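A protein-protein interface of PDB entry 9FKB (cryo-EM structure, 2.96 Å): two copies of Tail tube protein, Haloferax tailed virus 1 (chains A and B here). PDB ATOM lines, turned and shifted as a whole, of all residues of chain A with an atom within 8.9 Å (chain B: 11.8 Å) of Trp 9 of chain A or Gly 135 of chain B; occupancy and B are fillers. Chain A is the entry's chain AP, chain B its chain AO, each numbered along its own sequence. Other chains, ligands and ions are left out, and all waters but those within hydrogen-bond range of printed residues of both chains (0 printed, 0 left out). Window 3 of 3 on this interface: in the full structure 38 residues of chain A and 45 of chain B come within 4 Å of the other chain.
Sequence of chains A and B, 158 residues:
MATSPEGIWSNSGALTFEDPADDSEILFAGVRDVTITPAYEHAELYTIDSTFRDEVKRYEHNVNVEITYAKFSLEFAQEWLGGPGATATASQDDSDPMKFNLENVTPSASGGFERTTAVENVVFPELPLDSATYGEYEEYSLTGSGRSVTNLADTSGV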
ATOM      1  N   GLU A   6     -15.474  -0.205  24.590  1.00  0.00           N
ATOM      2  CA  GLU A   6     -15.897   0.405  23.331  1.00  0.00           C
ATOM      3  C   GLU A   6     -14.900   1.448  22.819  1.00  0.00           C
ATOM      4  O   GLU A   6     -14.185   2.083  23.595  1.00  0.00           O
ATOM      5  CB  GLU A   6     -17.285   1.010  23.529  1.00  0.00           C
ATOM      6  CG  GLU A   6     -18.183   0.883  22.319  1.00  0.00           C
ATOM      7  CD  GLU A   6     -19.657   0.832  22.703  1.00  0.00           C
ATOM      8  OE1 GLU A   6     -20.071   1.617  23.602  1.00  0.00           O
ATOM      9  OE2 GLU A   6     -20.404   0.032  22.081  1.00  0.00           O
ATOM     10  N   GLY A   7     -14.869   1.656  21.496  1.00  0.00           N
ATOM     11  CA  GLY A   7     -14.000   2.674  20.913  1.00  0.00           C
ATOM     12  C   GLY A   7     -14.510   4.095  21.178  1.00  0.00           C
ATOM     13  O   GLY A   7     -15.690   4.299  21.480  1.00  0.00           O
ATOM     14  N   ILE A   8     -13.611   5.075  21.055  1.00  0.00           N
ATOM     15  CA  ILE A   8     -13.966   6.469  21.308  1.00  0.00           C
ATOM     16  C   ILE A   8     -13.420   7.358  20.204  1.00  0.00           C
ATOM     17  O   ILE A   8     -12.223   7.331  19.935  1.00  0.00           O
ATOM     18  CB  ILE A   8     -13.480   6.915  22.703  1.00  0.00           C
ATOM     19  CG1 ILE A   8     -14.367   6.289  23.777  1.00  0.00           C
ATOM     20  CG2 ILE A   8     -13.477   8.426  22.856  1.00  0.00           C
ATOM     21  CD1 ILE A   8     -13.735   6.218  25.169  1.00  0.00           C
ATOM     22  N   TRP A   9     -14.304   8.153  19.586  1.00  0.00           N
ATOM     23  CA  TRP A   9     -13.887   9.149  18.616  1.00  0.00           C
ATOM     24  C   TRP A   9     -13.312  10.363  19.344  1.00  0.00           C
ATOM     25  O   TRP A   9     -14.021  10.975  20.132  1.00  0.00           O
ATOM     26  CB  TRP A   9     -15.096   9.499  17.735  1.00  0.00           C
ATOM     27  CG  TRP A   9     -14.801  10.474  16.639  1.00  0.00           C
ATOM     28  CD1 TRP A   9     -15.349  11.713  16.496  1.00  0.00           C
ATOM     29  CD2 TRP A   9     -13.910  10.304  15.507  1.00  0.00           C
ATOM     30  NE1 TRP A   9     -14.832  12.330  15.392  1.00  0.00           N
ATOM     31  CE2 TRP A   9     -13.909  11.516  14.781  1.00  0.00           C
ATOM     32  CE3 TRP A   9     -13.041   9.287  15.077  1.00  0.00           C
ATOM     33  CZ2 TRP A   9     -13.146  11.682  13.609  1.00  0.00           C
ATOM     34  CZ3 TRP A   9     -12.272   9.452  13.936  1.00  0.00           C
ATOM     35  CH2 TRP A   9     -12.338  10.638  13.199  1.00  0.00           C
ATOM     36  N   SER A  10     -12.044  10.732  19.088  1.00  0.00           N
ATOM     37  CA  SER A  10     -11.365  11.722  19.905  1.00  0.00           C
ATOM     38  C   SER A  10     -12.134  13.034  19.976  1.00  0.00           C
ATOM     39  O   SER A  10     -12.240  13.649  21.042  1.00  0.00           O
ATOM     40  CB  SER A  10      -9.970  11.961  19.430  1.00  0.00           C
ATOM     41  OG  SER A  10      -9.193  10.804  19.691  1.00  0.00           O
ATOM     42  N   ASN A  11     -12.609  13.492  18.821  1.00  0.00           N
ATOM     43  CA  ASN A  11     -13.192  14.811  18.686  1.00  0.00           C
ATOM     44  C   ASN A  11     -14.458  15.008  19.526  1.00  0.00           C
ATOM     45  O   ASN A  11     -14.871  16.146  19.765  1.00  0.00           O
ATOM     46  CB  ASN A  11     -13.501  15.098  17.230  1.00  0.00           C
ATOM     47  CG  ASN A  11     -12.322  14.977  16.288  1.00  0.00           C
ATOM     48  OD1 ASN A  11     -11.173  14.898  16.699  1.00  0.00           O
ATOM     49  ND2 ASN A  11     -12.595  14.964  14.997  1.00  0.00           N
ATOM     50  N   SER A  12     -15.096  13.920  19.960  1.00  0.00           N
ATOM     51  CA  SER A  12     -16.312  13.991  20.763  1.00  0.00           C
ATOM     52  C   SER A  12     -16.070  14.549  22.164  1.00  0.00           C
ATOM     53  O   SER A  12     -17.027  14.927  22.838  1.00  0.00           O
ATOM     54  CB  SER A  12     -16.925  12.640  20.867  1.00  0.00           C
ATOM     55  OG  SER A  12     -17.173  12.142  19.574  1.00  0.00           O
ATOM     56  N   GLY A  13     -14.814  14.564  22.628  1.00  0.00           N
ATOM     57  CA  GLY A  13     -14.499  14.983  23.984  1.00  0.00           C
ATOM     58  C   GLY A  13     -14.616  16.493  24.177  1.00  0.00           C
ATOM     59  O   GLY A  13     -14.036  17.271  23.421  1.00  0.00           O
ATOM     60  N   ALA A  14     -15.361  16.893  25.215  1.00  0.00           N
ATOM     61  CA  ALA A  14     -15.463  18.280  25.646  1.00  0.00           C
ATOM     62  C   ALA A  14     -14.607  18.500  26.901  1.00  0.00           C
ATOM     63  O   ALA A  14     -14.922  17.987  27.981  1.00  0.00           O
ATOM     64  CB  ALA A  14     -16.922  18.609  25.877  1.00  0.00           C
ATOM     65  N   VAL A  31      -8.154  22.161  21.323  1.00  0.00           N
ATOM     66  CA  VAL A  31      -7.211  21.063  21.515  1.00  0.00           C
ATOM     67  C   VAL A  31      -7.065  20.192  20.267  1.00  0.00           C
ATOM     68  O   VAL A  31      -7.965  20.069  19.446  1.00  0.00           O
ATOM     69  CB  VAL A  31      -7.549  20.208  22.748  1.00  0.00           C
ATOM     70  CG1 VAL A  31      -7.374  21.031  24.005  1.00  0.00           C
ATOM     71  CG2 VAL A  31      -8.951  19.622  22.730  1.00  0.00           C
ATOM     72  N   ARG A  32      -5.888  19.574  20.132  1.00  0.00           N
ATOM     73  CA  ARG A  32      -5.544  18.687  19.040  1.00  0.00           C
ATOM     74  C   ARG A  32      -5.141  17.308  19.564  1.00  0.00           C
ATOM     75  O   ARG A  32      -5.512  16.297  18.973  1.00  0.00           O
ATOM     76  CB  ARG A  32      -4.469  19.318  18.153  1.00  0.00           C
ATOM     77  CG  ARG A  32      -4.910  20.624  17.523  1.00  0.00           C
ATOM     78  CD  ARG A  32      -4.705  20.833  16.035  1.00  0.00           C
ATOM     79  NE  ARG A  32      -3.519  21.569  15.704  1.00  0.00           N
ATOM     80  CZ  ARG A  32      -3.479  22.630  14.892  1.00  0.00           C
ATOM     81  NH1 ARG A  32      -2.315  23.220  14.655  1.00  0.00           N
ATOM     82  NH2 ARG A  32      -4.590  23.094  14.339  1.00  0.00           N
ATOM     83  N   ASP A  33      -4.419  17.274  20.688  1.00  0.00           N
ATOM     84  CA  ASP A  33      -4.118  16.040  21.404  1.00  0.00           C
ATOM     85  C   ASP A  33      -4.434  16.251  22.883  1.00  0.00           C
ATOM     86  O   ASP A  33      -4.234  17.357  23.391  1.00  0.00           O
ATOM     87  CB  ASP A  33      -2.625  15.695  21.321  1.00  0.00           C
ATOM     88  CG  ASP A  33      -1.970  15.743  19.935  1.00  0.00           C
ATOM     89  OD1 ASP A  33      -2.513  15.100  19.001  1.00  0.00           O
ATOM     90  OD2 ASP A  33      -0.894  16.389  19.806  1.00  0.00           O
ATOM     91  N   ASN A 104     -12.895  16.485  31.588  1.00  0.00           N
ATOM     92  CA  ASN A 104     -13.084  16.109  30.201  1.00  0.00           C
ATOM     93  C   ASN A 104     -14.196  15.065  30.097  1.00  0.00           C
ATOM     94  O   ASN A 104     -14.141  14.044  30.782  1.00  0.00           O
ATOM     95  CB  ASN A 104     -11.785  15.574  29.613  1.00  0.00           C
ATOM     96  CG  ASN A 104     -11.903  15.335  28.123  1.00  0.00           C
ATOM     97  OD1 ASN A 104     -12.561  16.095  27.403  1.00  0.00           O
ATOM     98  ND2 ASN A 104     -11.304  14.256  27.641  1.00  0.00           N
ATOM     99  N   VAL A 105     -15.198  15.313  29.234  1.00  0.00           N
ATOM    100  CA  VAL A 105     -16.365  14.449  29.136  1.00  0.00           C
ATOM    101  C   VAL A 105     -16.466  13.934  27.706  1.00  0.00           C
ATOM    102  O   VAL A 105     -16.446  14.726  26.768  1.00  0.00           O
ATOM    103  CB  VAL A 105     -17.639  15.200  29.546  1.00  0.00           C
ATOM    104  CG1 VAL A 105     -18.825  14.252  29.577  1.00  0.00           C
ATOM    105  CG2 VAL A 105     -17.477  15.858  30.905  1.00  0.00           C
ATOM    106  N   THR A 106     -16.581  12.608  27.538  1.00  0.00           N
ATOM    107  CA  THR A 106     -16.443  12.010  26.217  1.00  0.00           C
ATOM    108  C   THR A 106     -17.389  10.820  26.031  1.00  0.00           C
ATOM    109  O   THR A 106     -17.257   9.815  26.717  1.00  0.00           O
ATOM    110  CB  THR A 106     -15.002  11.550  25.961  1.00  0.00           C
ATOM    111  OG1 THR A 106     -14.100  12.627  26.149  1.00  0.00           O
ATOM    112  CG2 THR A 106     -14.776  11.093  24.543  1.00  0.00           C
ATOM    113  N   PRO A 107     -18.355  10.886  25.083  1.00  0.00           N
ATOM    114  CA  PRO A 107     -19.152   9.721  24.709  1.00  0.00           C
ATOM    115  C   PRO A 107     -18.346   8.608  24.043  1.00  0.00           C
ATOM    116  O   PRO A 107     -17.370   8.855  23.327  1.00  0.00           O
ATOM    117  CB  PRO A 107     -20.162  10.276  23.703  1.00  0.00           C
ATOM    118  CG  PRO A 107     -20.224  11.762  24.034  1.00  0.00           C
ATOM    119  CD  PRO A 107     -18.799  12.102  24.400  1.00  0.00           C
ATOM    120  N   SER A 108     -18.802   7.365  24.253  1.00  0.00           N
ATOM    121  CA  SER A 108     -18.420   6.220  23.432  1.00  0.00           C
ATOM    122  C   SER A 108     -18.763   6.486  21.960  1.00  0.00           C
ATOM    123  O   SER A 108     -19.745   7.175  21.676  1.00  0.00           O
ATOM    124  CB  SER A 108     -19.123   4.982  23.956  1.00  0.00           C
ATOM    125  OG  SER A 108     -19.160   3.951  22.992  1.00  0.00           O
ATOM    126  N   ALA A 109     -18.037   5.844  21.027  1.00  0.00           N
ATOM    127  CA  ALA A 109     -18.364   5.867  19.603  1.00  0.00           C
ATOM    128  C   ALA A 109     -19.788   5.360  19.317  1.00  0.00           C
ATOM    129  O   ALA A 109     -20.471   5.875  18.436  1.00  0.00           O
ATOM    130  CB  ALA A 109     -17.340   5.077  18.843  1.00  0.00           C
ATOM    131  N   SER A 110     -20.257   4.349  20.063  1.00  0.00           N
ATOM    132  CA  SER A 110     -21.616   3.823  19.954  1.00  0.00           C
ATOM    133  C   SER A 110     -22.638   4.599  20.797  1.00  0.00           C
ATOM    134  O   SER A 110     -23.808   4.214  20.828  1.00  0.00           O
ATOM    135  CB  SER A 110     -21.687   2.380  20.406  1.00  0.00           C
ATOM    136  OG  SER A 110     -20.621   1.584  19.908  1.00  0.00           O
ATOM    137  N   GLY A 111     -22.222   5.607  21.574  1.00  0.00           N
ATOM    138  CA  GLY A 111     -23.061   6.229  22.600  1.00  0.00           C
ATOM    139  C   GLY A 111     -23.415   5.336  23.805  1.00  0.00           C
ATOM    140  O   GLY A 111     -24.191   5.750  24.672  1.00  0.00           O
ATOM    141  N   ARG A 115     -17.741   8.476  29.440  1.00  0.00           N
ATOM    142  CA  ARG A 115     -16.853   8.690  30.571  1.00  0.00           C
ATOM    143  C   ARG A 115     -16.683  10.184  30.848  1.00  0.00           C
ATOM    144  O   ARG A 115     -16.450  10.967  29.941  1.00  0.00           O
ATOM    145  CB  ARG A 115     -15.547   7.905  30.450  1.00  0.00           C
ATOM    146  CG  ARG A 115     -14.555   8.584  29.526  1.00  0.00           C
ATOM    147  CD  ARG A 115     -13.199   7.951  29.307  1.00  0.00           C
ATOM    148  NE  ARG A 115     -12.503   8.969  28.534  1.00  0.00           N
ATOM    149  CZ  ARG A 115     -11.723   8.683  27.500  1.00  0.00           C
ATOM    150  NH1 ARG A 115     -11.187   9.675  26.801  1.00  0.00           N
ATOM    151  NH2 ARG A 115     -11.418   7.420  27.225  1.00  0.00           N
ATOM    152  N   ARG B  32      -4.405  -4.011  19.863  1.00  0.00           N
ATOM    153  CA  ARG B  32      -3.730  -3.831  18.591  1.00  0.00           C
ATOM    154  C   ARG B  32      -2.374  -4.530  18.635  1.00  0.00           C
ATOM    155  O   ARG B  32      -2.017  -5.238  17.698  1.00  0.00           O
ATOM    156  CB  ARG B  32      -3.585  -2.347  18.269  1.00  0.00           C
ATOM    157  CG  ARG B  32      -4.901  -1.697  17.901  1.00  0.00           C
ATOM    158  CD  ARG B  32      -4.778  -0.245  17.471  1.00  0.00           C
ATOM    159  NE  ARG B  32      -6.026   0.228  16.895  1.00  0.00           N
ATOM    160  CZ  ARG B  32      -6.359   1.478  16.561  1.00  0.00           C
ATOM    161  NH1 ARG B  32      -7.554   1.702  16.043  1.00  0.00           N
ATOM    162  NH2 ARG B  32      -5.514   2.491  16.658  1.00  0.00           N
ATOM    163  N   TYR B  69      -4.043  -0.775  22.708  1.00  0.00           N
ATOM    164  CA  TYR B  69      -5.439  -1.131  22.504  1.00  0.00           C
ATOM    165  C   TYR B  69      -6.292   0.096  22.154  1.00  0.00           C
ATOM    166  O   TYR B  69      -5.851   1.243  22.298  1.00  0.00           O
ATOM    167  CB  TYR B  69      -5.943  -1.906  23.717  1.00  0.00           C
ATOM    168  CG  TYR B  69      -6.197  -1.119  24.978  1.00  0.00           C
ATOM    169  CD1 TYR B  69      -5.155  -0.624  25.759  1.00  0.00           C
ATOM    170  CD2 TYR B  69      -7.495  -0.896  25.418  1.00  0.00           C
ATOM    171  CE1 TYR B  69      -5.399   0.062  26.941  1.00  0.00           C
ATOM    172  CE2 TYR B  69      -7.753  -0.196  26.589  1.00  0.00           C
ATOM    173  CZ  TYR B  69      -6.705   0.284  27.358  1.00  0.00           C
ATOM    174  OH  TYR B  69      -6.981   0.975  28.509  1.00  0.00           O
ATOM    175  N   ALA B  70      -7.531  -0.147  21.684  1.00  0.00           N
ATOM    176  CA  ALA B  70      -8.344   0.904  21.083  1.00  0.00           C
ATOM    177  C   ALA B  70      -9.809   0.913  21.539  1.00  0.00           C
ATOM    178  O   ALA B  70     -10.548   1.826  21.166  1.00  0.00           O
ATOM    179  CB  ALA B  70      -8.203   0.819  19.582  1.00  0.00           C
ATOM    180  N   LYS B  71     -10.241  -0.063  22.356  1.00  0.00           N
ATOM    181  CA  LYS B  71     -11.545  -0.021  23.014  1.00  0.00           C
ATOM    182  C   LYS B  71     -11.356   0.294  24.504  1.00  0.00           C
ATOM    183  O   LYS B  71     -10.727  -0.474  25.215  1.00  0.00           O
ATOM    184  CB  LYS B  71     -12.321  -1.320  22.831  1.00  0.00           C
ATOM    185  CG  LYS B  71     -12.792  -1.541  21.403  1.00  0.00           C
ATOM    186  CD  LYS B  71     -13.698  -2.702  21.132  1.00  0.00           C
ATOM    187  CE  LYS B  71     -13.581  -3.250  19.699  1.00  0.00           C
ATOM    188  NZ  LYS B  71     -14.051  -4.659  19.461  1.00  0.00           N
ATOM    189  N   PHE B  72     -11.903   1.412  24.992  1.00  0.00           N
ATOM    190  CA  PHE B  72     -11.757   1.816  26.383  1.00  0.00           C
ATOM    191  C   PHE B  72     -12.650   0.965  27.286  1.00  0.00           C
ATOM    192  O   PHE B  72     -13.840   0.802  27.006  1.00  0.00           O
ATOM    193  CB  PHE B  72     -12.187   3.277  26.522  1.00  0.00           C
ATOM    194  CG  PHE B  72     -12.001   3.832  27.910  1.00  0.00           C
ATOM    195  CD1 PHE B  72     -10.751   4.271  28.328  1.00  0.00           C
ATOM    196  CD2 PHE B  72     -13.064   3.887  28.806  1.00  0.00           C
ATOM    197  CE1 PHE B  72     -10.575   4.750  29.620  1.00  0.00           C
ATOM    198  CE2 PHE B  72     -12.885   4.353  30.098  1.00  0.00           C
ATOM    199  CZ  PHE B  72     -11.642   4.790  30.497  1.00  0.00           C
ATOM    200  N   LEU B 129      -6.066   7.194  30.735  1.00  0.00           N
ATOM    201  CA  LEU B 129      -7.510   7.354  30.689  1.00  0.00           C
ATOM    202  C   LEU B 129      -7.911   7.965  29.352  1.00  0.00           C
ATOM    203  O   LEU B 129      -8.423   7.261  28.488  1.00  0.00           O
ATOM    204  CB  LEU B 129      -7.976   8.210  31.863  1.00  0.00           C
ATOM    205  CG  LEU B 129      -7.833   7.527  33.222  1.00  0.00           C
ATOM    206  CD1 LEU B 129      -8.461   8.422  34.285  1.00  0.00           C
ATOM    207  CD2 LEU B 129      -8.454   6.118  33.263  1.00  0.00           C
ATOM    208  N   ASP B 130      -7.624   9.258  29.173  1.00  0.00           N
ATOM    209  CA  ASP B 130      -7.802   9.909  27.886  1.00  0.00           C
ATOM    210  C   ASP B 130      -6.512   9.808  27.073  1.00  0.00           C
ATOM    211  O   ASP B 130      -5.409   9.913  27.608  1.00  0.00           O
ATOM    212  CB  ASP B 130      -8.204  11.371  28.080  1.00  0.00           C
ATOM    213  CG  ASP B 130      -9.522  11.613  28.810  1.00  0.00           C
ATOM    214  OD1 ASP B 130     -10.280  10.666  29.072  1.00  0.00           O
ATOM    215  OD2 ASP B 130      -9.797  12.788  29.108  1.00  0.00           O
ATOM    216  N   SER B 131      -6.656   9.644  25.757  1.00  0.00           N
ATOM    217  CA  SER B 131      -5.541   9.530  24.832  1.00  0.00           C
ATOM    218  C   SER B 131      -5.977   9.989  23.441  1.00  0.00           C
ATOM    219  O   SER B 131      -5.962   9.231  22.465  1.00  0.00           O
ATOM    220  CB  SER B 131      -5.011   8.116  24.840  1.00  0.00           C
ATOM    221  OG  SER B 131      -3.793   8.039  24.108  1.00  0.00           O
ATOM    222  N   ALA B 132      -6.467  11.231  23.393  1.00  0.00           N
ATOM    223  CA  ALA B 132      -7.114  11.831  22.238  1.00  0.00           C
ATOM    224  C   ALA B 132      -6.102  12.357  21.234  1.00  0.00           C
ATOM    225  O   ALA B 132      -5.133  13.008  21.613  1.00  0.00           O
ATOM    226  CB  ALA B 132      -7.965  12.964  22.741  1.00  0.00           C
ATOM    227  N   THR B 133      -6.414  12.153  19.943  1.00  0.00           N
ATOM    228  CA  THR B 133      -5.822  12.878  18.822  1.00  0.00           C
ATOM    229  C   THR B 133      -6.946  13.279  17.869  1.00  0.00           C
ATOM    230  O   THR B 133      -7.740  12.431  17.457  1.00  0.00           O
ATOM    231  CB  THR B 133      -4.815  12.005  18.062  1.00  0.00           C
ATOM    232  OG1 THR B 133      -3.786  11.565  18.947  1.00  0.00           O
ATOM    233  CG2 THR B 133      -4.196  12.691  16.862  1.00  0.00           C
ATOM    234  N   TYR B 134      -7.002  14.557  17.481  1.00  0.00           N
ATOM    235  CA  TYR B 134      -8.086  15.027  16.629  1.00  0.00           C
ATOM    236  C   TYR B 134      -8.116  14.309  15.280  1.00  0.00           C
ATOM    237  O   TYR B 134      -7.082  14.069  14.665  1.00  0.00           O
ATOM    238  CB  TYR B 134      -8.099  16.548  16.478  1.00  0.00           C
ATOM    239  CG  TYR B 134      -7.146  17.146  15.474  1.00  0.00           C
ATOM    240  CD1 TYR B 134      -5.775  16.953  15.572  1.00  0.00           C
ATOM    241  CD2 TYR B 134      -7.604  17.976  14.469  1.00  0.00           C
ATOM    242  CE1 TYR B 134      -4.884  17.528  14.676  1.00  0.00           C
ATOM    243  CE2 TYR B 134      -6.727  18.572  13.571  1.00  0.00           C
ATOM    244  CZ  TYR B 134      -5.362  18.344  13.665  1.00  0.00           C
ATOM    245  OH  TYR B 134      -4.484  18.918  12.780  1.00  0.00           O
ATOM    246  N   GLY B 135      -9.330  13.932  14.858  1.00  0.00           N
ATOM    247  CA  GLY B 135      -9.534  13.204  13.617  1.00  0.00           C
ATOM    248  C   GLY B 135      -9.086  11.741  13.685  1.00  0.00           C
ATOM    249  O   GLY B 135      -8.894  11.107  12.645  1.00  0.00           O
ATOM    250  N   GLU B 136      -8.992  11.179  14.898  1.00  0.00           N
ATOM    251  CA  GLU B 136      -8.745   9.750  15.082  1.00  0.00           C
ATOM    252  C   GLU B 136      -9.554   9.180  16.246  1.00  0.00           C
ATOM    253  O   GLU B 136      -9.967   9.894  17.163  1.00  0.00           O
ATOM    254  CB  GLU B 136      -7.275   9.480  15.379  1.00  0.00           C
ATOM    255  CG  GLU B 136      -6.309  10.024  14.337  1.00  0.00           C
ATOM    256  CD  GLU B 136      -4.884   9.522  14.479  1.00  0.00           C
ATOM    257  OE1 GLU B 136      -4.440   9.309  15.627  1.00  0.00           O
ATOM    258  OE2 GLU B 136      -4.215   9.334  13.434  1.00  0.00           O
ATOM    259  N   TYR B 137      -9.716   7.855  16.240  1.00  0.00           N
ATOM    260  CA  TYR B 137     -10.163   7.190  17.451  1.00  0.00           C
ATOM    261  C   TYR B 137      -9.027   7.150  18.474  1.00  0.00           C
ATOM    262  O   TYR B 137      -7.869   7.008  18.094  1.00  0.00           O
ATOM    263  CB  TYR B 137     -10.681   5.791  17.130  1.00  0.00           C
ATOM    264  CG  TYR B 137     -11.932   5.824  16.293  1.00  0.00           C
ATOM    265  CD1 TYR B 137     -13.181   5.970  16.878  1.00  0.00           C
ATOM    266  CD2 TYR B 137     -11.859   5.794  14.913  1.00  0.00           C
ATOM    267  CE1 TYR B 137     -14.337   6.033  16.113  1.00  0.00           C
ATOM    268  CE2 TYR B 137     -13.007   5.836  14.132  1.00  0.00           C
ATOM    269  CZ  TYR B 137     -14.250   5.958  14.733  1.00  0.00           C
ATOM    270  OH  TYR B 137     -15.382   6.005  13.963  1.00  0.00           O
ATOM    271  N   GLU B 138      -9.372   7.232  19.770  1.00  0.00           N
ATOM    272  CA  GLU B 138      -8.382   7.141  20.841  1.00  0.00           C
ATOM    273  C   GLU B 138      -7.675   5.778  20.836  1.00  0.00           C
ATOM    274  O   GLU B 138      -8.295   4.736  20.637  1.00  0.00           O
ATOM    275  CB  GLU B 138      -9.027   7.299  22.213  1.00  0.00           C
ATOM    276  CG  GLU B 138      -9.458   8.717  22.575  1.00  0.00           C
ATOM    277  CD  GLU B 138      -9.695   8.879  24.073  1.00  0.00           C
ATOM    278  OE1 GLU B 138     -10.314   7.978  24.682  1.00  0.00           O
ATOM    279  OE2 GLU B 138      -9.274   9.895  24.649  1.00  0.00           O
ATOM    280  N   GLU B 139      -6.360   5.805  21.084  1.00  0.00           N
ATOM    281  CA  GLU B 139      -5.538   4.609  21.213  1.00  0.00           C
ATOM    282  C   GLU B 139      -4.690   4.725  22.476  1.00  0.00           C
ATOM    283  O   GLU B 139      -4.161   5.793  22.788  1.00  0.00           O
ATOM    284  CB  GLU B 139      -4.665   4.460  19.972  1.00  0.00           C
ATOM    285  CG  GLU B 139      -3.754   3.252  20.001  1.00  0.00           C
ATOM    286  CD  GLU B 139      -2.797   3.255  18.823  1.00  0.00           C
ATOM    287  OE1 GLU B 139      -1.797   4.012  18.888  1.00  0.00           O
ATOM    288  OE2 GLU B 139      -3.074   2.527  17.826  1.00  0.00           O
ATOM    289  N   TYR B 140      -4.582   3.616  23.221  1.00  0.00           N
ATOM    290  CA  TYR B 140      -4.010   3.616  24.556  1.00  0.00           C
ATOM    291  C   TYR B 140      -2.865   2.611  24.647  1.00  0.00           C
ATOM    292  O   TYR B 140      -2.951   1.508  24.110  1.00  0.00           O
ATOM    293  CB  TYR B 140      -5.074   3.224  25.575  1.00  0.00           C
ATOM    294  CG  TYR B 140      -6.426   3.844  25.348  1.00  0.00           C
ATOM    295  CD1 TYR B 140      -6.738   5.112  25.834  1.00  0.00           C
ATOM    296  CD2 TYR B 140      -7.391   3.152  24.630  1.00  0.00           C
ATOM    297  CE1 TYR B 140      -7.985   5.686  25.604  1.00  0.00           C
ATOM    298  CE2 TYR B 140      -8.640   3.711  24.403  1.00  0.00           C
ATOM    299  CZ  TYR B 140      -8.940   4.977  24.892  1.00  0.00           C
ATOM    300  OH  TYR B 140     -10.185   5.498  24.674  1.00  0.00           O
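N of Phe 72 of chain B sits at hydrogen-bond distance from O of Glu 6 of chain A (2.8 Å). The backbone carbonyl oxygen (O) of Leu 129 of chain B is in hydrogen-bond range of the guanidinium group (NH2) of Arg 115 of chain A, at 3.3 Å. The side-chain amide nitrogen (ND2) of Asn 104 of chain A is in hydrogen-bond range of the side-chain carboxylate (OD2) of Asp 130 of chain B, at 2.6 Å. The side-chain carboxylate (OD1) of Asp 130 of chain B lies within salt-bridge range of the guanidinium group (NH1) of Arg 115 of chain A (2.6 Å). N of Thr 133 of chain B lies within hydrogen-bond range of OG of Ser 10 of chain A (3.1 Å). The backbone NH (N) of Tyr 134 of chain B lies within hydrogen-bond range of the backbone carbonyl oxygen (O) of Arg 32 of chain A (2.7 Å). N of Gly 135 of chain B is in hydrogen-bond range of OD1 of Asn 11 of chain A, 2.8 Å away. The backbone carbonyl oxygen of Glu 136 of chain B sits at hydrogen-bond distance from the side-chain hydroxyl of Ser 10 of chain A (2.8 Å). The backbone NH of Glu 138 of chain B lies within hydrogen-bond range of the backbone carbonyl oxygen of Ile 8 of chain A (2.9 Å). The guanidinium group of Arg 115 of chain A lies within salt-bridge range of the side-chain carboxylate of Glu 138 of chain B (2.8 Å). The guanidinium group (NH2) of Arg 115 of chain A sits at hydrogen-bond distance from the side-chain hydroxyl (OH) of Tyr 140 of chain B, 3.4 Å away.
N of Tyr 140 of chain B is in hydrogen-bond range of O of Tyr 69 of chain B (2.8 Å). The backbone carbonyl oxygen (O) of Gly 7 of chain A lies within hydrogen-bond range of the backbone NH (N) of Ala 109 of chain A, at 2.8 Å.
Lys 71 of chain B touches Glu 6 of chain A (CA to O, 3.4 Å). Ser 10 of chain A touches Ala 132 of chain B. OG of Ser 10 of chain A touches CG of Glu 138 of chain B, at 3.6 Å. Asp 33 of chain A touches Ala 132 of chain B (CA to O, 3.2 Å).
Gly 135 of chain B touches just these residues of chain A: Trp 9 (3.5 Å) and Asn 11 (2.8 Å). Of chain B, only Phe 72 (3.6 Å), Tyr 137 (3.2 Å), Glu 138 (2.9 Å) and Tyr 140 (3.7 Å) come within 4 Å of Ile 8 of chain A. Printed residues of chain A within 4 Å of Glu 138 of chain B: Ile 8 (2.9 Å), Ser 10 (3.6 Å) and Arg 115 (2.8 Å). Printed residues of chain A within 4 Å of Tyr 134 of chain B: Asn 11 and Arg 32. Of the printed residues of chain A, Glu 136 of chain B touches Trp 9 and Ser 10. The nearest residue of chain B that does not touch Trp 9 of chain A is Glu 138 of chain B (5.0 Å). The nearest residue of chain A that does not touch Gly 135 of chain B is Ser 10 of chain A (5.0 Å).
Hydrophobic or aromatic side chains of chain A that line the printed part of chain B: Ile 8 and Trp 9. Of the 17 printed residues of chain B, 13 touch a printed residue of chain A. Printed residues of chain B that touch a printed residue of chain A: Ala 70, Lys 71, Phe 72, Leu 129, Asp 130, Ala 132, Thr 133, Tyr 134, Gly 135, Glu 136, Tyr 137, Glu 138 and Tyr 140. Among the printed residues, Asp or Glu carboxylates within 4 Å of a Lys or Arg side-chain nitrogen of the other chain: Arg 115 of chain A with Asp 130 of chain B (2.6 Å) and Arg 115 of chain A with Glu 138 of chain B (2.8 Å).
1 position is printed for both chains. Of the 28 pairs that touch across the chains among the printed residues, none has its exchanged pair printed and touching as well.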
